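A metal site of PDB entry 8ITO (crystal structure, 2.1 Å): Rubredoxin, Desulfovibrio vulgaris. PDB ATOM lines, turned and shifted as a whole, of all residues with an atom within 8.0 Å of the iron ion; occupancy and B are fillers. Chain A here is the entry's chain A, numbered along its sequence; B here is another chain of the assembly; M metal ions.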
ATOM      1  N   ARG A   9     -11.977 -28.180 -10.006  1.00  0.00           N
ATOM      2  CA  ARG A   9     -13.100 -27.326 -10.370  1.00  0.00           C
ATOM      3  C   ARG A   9     -14.417 -28.033 -10.137  1.00  0.00           C
ATOM      4  O   ARG A   9     -14.602 -29.194 -10.545  1.00  0.00           O
ATOM      5  CB  ARG A   9     -12.997 -26.904 -11.827  1.00  0.00           C
ATOM      6  CG  ARG A   9     -13.898 -25.735 -12.165  1.00  0.00           C
ATOM      7  CD  ARG A   9     -13.925 -25.497 -13.675  1.00  0.00           C
ATOM      8  NE  ARG A   9     -14.903 -24.492 -14.048  1.00  0.00           N
ATOM      9  CZ  ARG A   9     -14.618 -23.189 -14.130  1.00  0.00           C
ATOM     10  NH1 ARG A   9     -13.387 -22.738 -13.921  1.00  0.00           N
ATOM     11  NH2 ARG A   9     -15.584 -22.348 -14.451  1.00  0.00           N
ATOM     12  N   CYS A  10     -15.347 -27.336  -9.493  1.00  0.00           N
ATOM     13  CA  CYS A  10     -16.701 -27.835  -9.309  1.00  0.00           C
ATOM     14  C   CYS A  10     -17.426 -27.924 -10.647  1.00  0.00           C
ATOM     15  O   CYS A  10     -17.465 -26.957 -11.403  1.00  0.00           O
ATOM     16  CB  CYS A  10     -17.494 -26.945  -8.374  1.00  0.00           C
ATOM     17  SG  CYS A  10     -19.130 -27.596  -8.054  1.00  0.00           S
ATOM     18  N   GLN A  11     -18.042 -29.073 -10.917  1.00  0.00           N
ATOM     19  CA  GLN A  11     -18.588 -29.326 -12.242  1.00  0.00           C
ATOM     20  C   GLN A  11     -20.086 -29.098 -12.358  1.00  0.00           C
ATOM     21  O   GLN A  11     -20.622 -29.237 -13.458  1.00  0.00           O
ATOM     22  CB  GLN A  11     -18.246 -30.764 -12.685  1.00  0.00           C
ATOM     23  CG  GLN A  11     -16.762 -31.009 -12.979  1.00  0.00           C
ATOM     24  CD  GLN A  11     -16.168 -30.051 -14.008  1.00  0.00           C
ATOM     25  OE1 GLN A  11     -16.597 -30.003 -15.157  1.00  0.00           O
ATOM     26  NE2 GLN A  11     -15.176 -29.272 -13.582  1.00  0.00           N
ATOM     27  N   THR A  12     -20.796 -28.750 -11.276  1.00  0.00           N
ATOM     28  CA  THR A  12     -22.229 -28.554 -11.427  1.00  0.00           C
ATOM     29  C   THR A  12     -22.509 -27.444 -12.434  1.00  0.00           C
ATOM     30  O   THR A  12     -21.674 -26.552 -12.665  1.00  0.00           O
ATOM     31  CB  THR A  12     -22.923 -28.260 -10.090  1.00  0.00           C
ATOM     32  OG1 THR A  12     -22.777 -26.883  -9.747  1.00  0.00           O
ATOM     33  CG2 THR A  12     -22.364 -29.137  -8.971  1.00  0.00           C
ATOM     34  N   VAL A  13     -23.677 -27.512 -13.058  1.00  0.00           N
ATOM     35  CA  VAL A  13     -23.904 -26.806 -14.310  1.00  0.00           C
ATOM     36  C   VAL A  13     -23.787 -25.289 -14.151  1.00  0.00           C
ATOM     37  O   VAL A  13     -23.324 -24.596 -15.077  1.00  0.00           O
ATOM     38  CB  VAL A  13     -25.269 -27.228 -14.885  1.00  0.00           C
ATOM     39  CG1 VAL A  13     -26.380 -26.969 -13.848  1.00  0.00           C
ATOM     40  CG2 VAL A  13     -25.560 -26.469 -16.178  1.00  0.00           C
ATOM     41  N   ASN A  14     -24.185 -24.726 -13.012  1.00  0.00           N
ATOM     42  CA  ASN A  14     -24.182 -23.277 -12.835  1.00  0.00           C
ATOM     43  C   ASN A  14     -23.112 -22.797 -11.854  1.00  0.00           C
ATOM     44  O   ASN A  14     -23.170 -21.652 -11.386  1.00  0.00           O
ATOM     45  CB  ASN A  14     -25.566 -22.782 -12.400  1.00  0.00           C
ATOM     46  CG  ASN A  14     -26.524 -22.570 -13.585  1.00  0.00           C
ATOM     47  OD1 ASN A  14     -26.304 -23.117 -14.661  1.00  0.00           O
ATOM     48  ND2 ASN A  14     -27.580 -21.790 -13.385  1.00  0.00           N
ATOM     49  N   CYS A  15     -22.128 -23.651 -11.536  1.00  0.00           N
ATOM     50  CA  CYS A  15     -21.083 -23.250 -10.611  1.00  0.00           C
ATOM     51  C   CYS A  15     -19.785 -22.988 -11.364  1.00  0.00           C
ATOM     52  O   CYS A  15     -19.800 -22.459 -12.474  1.00  0.00           O
ATOM     53  CB  CYS A  15     -20.885 -24.320  -9.542  1.00  0.00           C
ATOM     54  SG  CYS A  15     -19.894 -23.739  -8.163  1.00  0.00           S
ATOM     55  N   GLY A  16     -18.644 -23.343 -10.778  1.00  0.00           N
ATOM     56  CA  GLY A  16     -17.372 -23.000 -11.394  1.00  0.00           C
ATOM     57  C   GLY A  16     -16.347 -22.542 -10.386  1.00  0.00           C
ATOM     58  O   GLY A  16     -15.334 -21.936 -10.726  1.00  0.00           O
ATOM     59  N   TYR A  17     -16.636 -22.809  -9.114  1.00  0.00           N
ATOM     60  CA  TYR A  17     -15.627 -22.669  -8.078  1.00  0.00           C
ATOM     61  C   TYR A  17     -14.457 -23.594  -8.357  1.00  0.00           C
ATOM     62  O   TYR A  17     -14.650 -24.721  -8.826  1.00  0.00           O
ATOM     63  CB  TYR A  17     -16.220 -23.027  -6.719  1.00  0.00           C
ATOM     64  CG  TYR A  17     -15.222 -22.930  -5.578  1.00  0.00           C
ATOM     65  CD1 TYR A  17     -14.915 -21.700  -5.001  1.00  0.00           C
ATOM     66  CD2 TYR A  17     -14.609 -24.078  -5.058  1.00  0.00           C
ATOM     67  CE1 TYR A  17     -14.028 -21.600  -3.915  1.00  0.00           C
ATOM     68  CE2 TYR A  17     -13.708 -24.004  -3.982  1.00  0.00           C
ATOM     69  CZ  TYR A  17     -13.420 -22.756  -3.426  1.00  0.00           C
ATOM     70  OH  TYR A  17     -12.535 -22.676  -2.365  1.00  0.00           O
ATOM     71  N   VAL A  18     -13.255 -23.109  -8.078  1.00  0.00           N
ATOM     72  CA  VAL A  18     -12.028 -23.900  -8.169  1.00  0.00           C
ATOM     73  C   VAL A  18     -11.423 -23.974  -6.772  1.00  0.00           C
ATOM     74  O   VAL A  18     -11.100 -22.929  -6.189  1.00  0.00           O
ATOM     75  CB  VAL A  18     -11.012 -23.297  -9.155  1.00  0.00           C
ATOM     76  CG1 VAL A  18      -9.743 -24.108  -9.123  1.00  0.00           C
ATOM     77  CG2 VAL A  18     -11.589 -23.248 -10.570  1.00  0.00           C
ATOM     78  N   TRP A  43     -17.044 -31.878   3.652  1.00  0.00           N
ATOM     79  CA  TRP A  43     -16.765 -30.635   2.926  1.00  0.00           C
ATOM     80  C   TRP A  43     -17.628 -30.541   1.693  1.00  0.00           C
ATOM     81  O   TRP A  43     -17.808 -31.526   0.955  1.00  0.00           O
ATOM     82  CB  TRP A  43     -15.290 -30.551   2.521  1.00  0.00           C
ATOM     83  CG  TRP A  43     -14.886 -29.281   1.785  1.00  0.00           C
ATOM     84  CD1 TRP A  43     -14.417 -28.116   2.341  1.00  0.00           C
ATOM     85  CD2 TRP A  43     -14.885 -29.067   0.365  1.00  0.00           C
ATOM     86  NE1 TRP A  43     -14.142 -27.192   1.361  1.00  0.00           N
ATOM     87  CE2 TRP A  43     -14.416 -27.751   0.143  1.00  0.00           C
ATOM     88  CE3 TRP A  43     -15.231 -29.861  -0.735  1.00  0.00           C
ATOM     89  CZ2 TRP A  43     -14.282 -27.211  -1.144  1.00  0.00           C
ATOM     90  CZ3 TRP A  43     -15.106 -29.312  -2.015  1.00  0.00           C
ATOM     91  CH2 TRP A  43     -14.642 -28.005  -2.202  1.00  0.00           C
ATOM     92  N   ARG A  44     -18.176 -29.356   1.459  1.00  0.00           N
ATOM     93  CA  ARG A  44     -18.976 -29.071   0.280  1.00  0.00           C
ATOM     94  C   ARG A  44     -18.393 -27.851  -0.438  1.00  0.00           C
ATOM     95  O   ARG A  44     -17.694 -27.031   0.149  1.00  0.00           O
ATOM     96  CB  ARG A  44     -20.443 -28.807   0.655  1.00  0.00           C
ATOM     97  CG  ARG A  44     -21.040 -29.845   1.598  1.00  0.00           C
ATOM     98  CD  ARG A  44     -21.079 -31.223   0.970  1.00  0.00           C
ATOM     99  NE  ARG A  44     -22.150 -32.062   1.495  1.00  0.00           N
ATOM    100  CZ  ARG A  44     -23.416 -31.990   1.107  1.00  0.00           C
ATOM    101  NH1 ARG A  44     -23.845 -31.038   0.286  1.00  0.00           N
ATOM    102  NH2 ARG A  44     -24.288 -32.903   1.552  1.00  0.00           N
ATOM    103  N   CYS A  45     -18.688 -27.762  -1.744  1.00  0.00           N
ATOM    104  CA  CYS A  45     -18.406 -26.559  -2.506  1.00  0.00           C
ATOM    105  C   CYS A  45     -18.962 -25.339  -1.780  1.00  0.00           C
ATOM    106  O   CYS A  45     -20.150 -25.319  -1.425  1.00  0.00           O
ATOM    107  CB  CYS A  45     -19.012 -26.661  -3.903  1.00  0.00           C
ATOM    108  SG  CYS A  45     -18.698 -25.214  -4.933  1.00  0.00           S
ATOM    109  N   PRO A  46     -18.140 -24.315  -1.511  1.00  0.00           N
ATOM    110  CA  PRO A  46     -18.674 -23.125  -0.825  1.00  0.00           C
ATOM    111  C   PRO A  46     -19.665 -22.348  -1.669  1.00  0.00           C
ATOM    112  O   PRO A  46     -20.444 -21.555  -1.107  1.00  0.00           O
ATOM    113  CB  PRO A  46     -17.423 -22.275  -0.525  1.00  0.00           C
ATOM    114  CG  PRO A  46     -16.361 -22.779  -1.427  1.00  0.00           C
ATOM    115  CD  PRO A  46     -16.713 -24.177  -1.858  1.00  0.00           C
ATOM    116  N   ILE A  47     -19.670 -22.519  -2.986  1.00  0.00           N
ATOM    117  CA  ILE A  47     -20.625 -21.802  -3.823  1.00  0.00           C
ATOM    118  C   ILE A  47     -21.933 -22.586  -3.883  1.00  0.00           C
ATOM    119  O   ILE A  47     -22.961 -22.144  -3.356  1.00  0.00           O
ATOM    120  CB  ILE A  47     -20.068 -21.535  -5.221  1.00  0.00           C
ATOM    121  CG1 ILE A  47     -18.894 -20.560  -5.127  1.00  0.00           C
ATOM    122  CG2 ILE A  47     -21.182 -20.943  -6.139  1.00  0.00           C
ATOM    123  CD1 ILE A  47     -18.308 -20.145  -6.478  1.00  0.00           C
ATOM    124  N   CYS A  48     -21.917 -23.771  -4.502  1.00  0.00           N
ATOM    125  CA  CYS A  48     -23.147 -24.495  -4.800  1.00  0.00           C
ATOM    126  C   CYS A  48     -23.461 -25.614  -3.804  1.00  0.00           C
ATOM    127  O   CYS A  48     -24.537 -26.218  -3.910  1.00  0.00           O
ATOM    128  CB  CYS A  48     -23.107 -25.064  -6.224  1.00  0.00           C
ATOM    129  SG  CYS A  48     -22.024 -26.517  -6.391  1.00  0.00           S
ATOM    130  N   LYS A  49     -22.562 -25.893  -2.870  1.00  0.00           N
ATOM    131  CA  LYS A  49     -22.710 -26.919  -1.832  1.00  0.00           C
ATOM    132  C   LYS A  49     -22.691 -28.351  -2.365  1.00  0.00           C
ATOM    133  O   LYS A  49     -23.067 -29.259  -1.621  1.00  0.00           O
ATOM    134  CB  LYS A  49     -23.974 -26.694  -0.993  1.00  0.00           C
ATOM    135  CG  LYS A  49     -23.876 -25.433  -0.132  1.00  0.00           C
ATOM    136  CD  LYS A  49     -22.883 -25.613   0.999  1.00  0.00           C
ATOM    137  CE  LYS A  49     -23.283 -24.831   2.250  1.00  0.00           C
ATOM    138  NZ  LYS A  49     -22.117 -24.686   3.179  1.00  0.00           N
ATOM    139  N   ALA A  50     -22.258 -28.584  -3.602  1.00  0.00           N
ATOM    140  CA  ALA A  50     -22.029 -29.950  -4.055  1.00  0.00           C
ATOM    141  C   ALA A  50     -20.979 -30.641  -3.177  1.00  0.00           C
ATOM    142  O   ALA A  50     -20.120 -29.996  -2.574  1.00  0.00           O
ATOM    143  CB  ALA A  50     -21.539 -29.950  -5.508  1.00  0.00           C
ATOM    144  N   THR A  51     -21.059 -31.975  -3.116  1.00  0.00           N
ATOM    145  CA  THR A  51     -20.022 -32.767  -2.469  1.00  0.00           C
ATOM    146  C   THR A  51     -18.775 -32.778  -3.338  1.00  0.00           C
ATOM    147  O   THR A  51     -18.775 -32.282  -4.476  1.00  0.00           O
ATOM    148  CB  THR A  51     -20.460 -34.211  -2.231  1.00  0.00           C
ATOM    149  OG1 THR A  51     -20.488 -34.914  -3.494  1.00  0.00           O
ATOM    150  CG2 THR A  51     -21.827 -34.285  -1.534  1.00  0.00           C
ATOM    151  N   CYS A  54     -18.415 -33.957  -7.150  1.00  0.00           N
ATOM    152  CA  CYS A  54     -18.731 -33.092  -8.272  1.00  0.00           C
ATOM    153  C   CYS A  54     -17.516 -32.335  -8.790  1.00  0.00           C
ATOM    154  O   CYS A  54     -17.668 -31.475  -9.664  1.00  0.00           O
ATOM    155  CB  CYS A  54     -19.840 -32.120  -7.887  1.00  0.00           C
ATOM    156  SG  CYS A  54     -21.451 -32.903  -7.539  1.00  0.00           S
ATOM    157  N   PHE A  55     -16.311 -32.631  -8.300  1.00  0.00           N
ATOM    158  CA  PHE A  55     -15.111 -31.895  -8.668  1.00  0.00           C
ATOM    159  C   PHE A  55     -14.180 -32.723  -9.561  1.00  0.00           C
ATOM    160  O   PHE A  55     -14.171 -33.947  -9.518  1.00  0.00           O
ATOM    161  CB  PHE A  55     -14.357 -31.456  -7.415  1.00  0.00           C
ATOM    162  CG  PHE A  55     -14.979 -30.289  -6.716  1.00  0.00           C
ATOM    163  CD1 PHE A  55     -16.119 -30.453  -5.957  1.00  0.00           C
ATOM    164  CD2 PHE A  55     -14.418 -29.016  -6.823  1.00  0.00           C
ATOM    165  CE1 PHE A  55     -16.699 -29.374  -5.314  1.00  0.00           C
ATOM    166  CE2 PHE A  55     -15.005 -27.936  -6.192  1.00  0.00           C
ATOM    167  CZ  PHE A  55     -16.141 -28.117  -5.436  1.00  0.00           C
ATOM    168  N   MET A  71     -25.439 -33.647  -8.277  1.00  0.00           N
ATOM    169  CA  MET A  71     -26.188 -32.543  -8.856  1.00  0.00           C
ATOM    170  C   MET A  71     -25.999 -32.501 -10.369  1.00  0.00           C
ATOM    171  O   MET A  71     -25.083 -33.138 -10.909  1.00  0.00           O
ATOM    172  CB  MET A  71     -25.759 -31.210  -8.224  1.00  0.00           C
ATOM    173  CG  MET A  71     -26.018 -31.085  -6.727  1.00  0.00           C
ATOM    174  SD  MET A  71     -25.164 -29.670  -5.924  1.00  0.00           S
ATOM    175  CE  MET A  71     -25.513 -28.314  -7.035  1.00  0.00           C
ATOM    176  N   ILE B  47     -22.317 -16.143 -12.574  1.00  0.00           N
ATOM    177  CA  ILE B  47     -23.008 -16.400 -11.324  1.00  0.00           C
ATOM    178  C   ILE B  47     -23.562 -15.129 -10.729  1.00  0.00           C
ATOM    179  O   ILE B  47     -24.754 -15.067 -10.403  1.00  0.00           O
ATOM    180  CB  ILE B  47     -22.108 -17.129 -10.312  1.00  0.00           C
ATOM    181  CG1 ILE B  47     -21.675 -18.497 -10.843  1.00  0.00           C
ATOM    182  CG2 ILE B  47     -22.900 -17.357  -9.031  1.00  0.00           C
ATOM    183  CD1 ILE B  47     -20.905 -19.347  -9.814  1.00  0.00           C
HETATM  184 FE    FE M   1     -19.975 -25.743  -6.856  1.00  0.00          FE
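The iron ion is bound by the side-chain sulfur of Cys 48, the side-chain sulfur of Cys 10, the side-chain sulfur of Cys 45 and the side-chain sulfur of Cys 15.
Of the 23 residues printed, 4 come within 4 Å of the iron ion.
The side-chain hydroxyl (OG1) of Thr 12 lies close to the side-chain sulfur (SG) of Cys 48 (3.5 Å). N of Cys 45 sits at hydrogen-bond distance from O of Ala 50 (2.8 Å). SG of Cys 48 sits close to N of Ala 50 (3.5 Å). O of Tyr 17 lies within hydrogen-bond range of N of Cys 10. SG of Cys 15 lies close to N of Tyr 17. SG of Cys 45 lies close to N of Ile 47 of chain A, at 3.5 Å.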
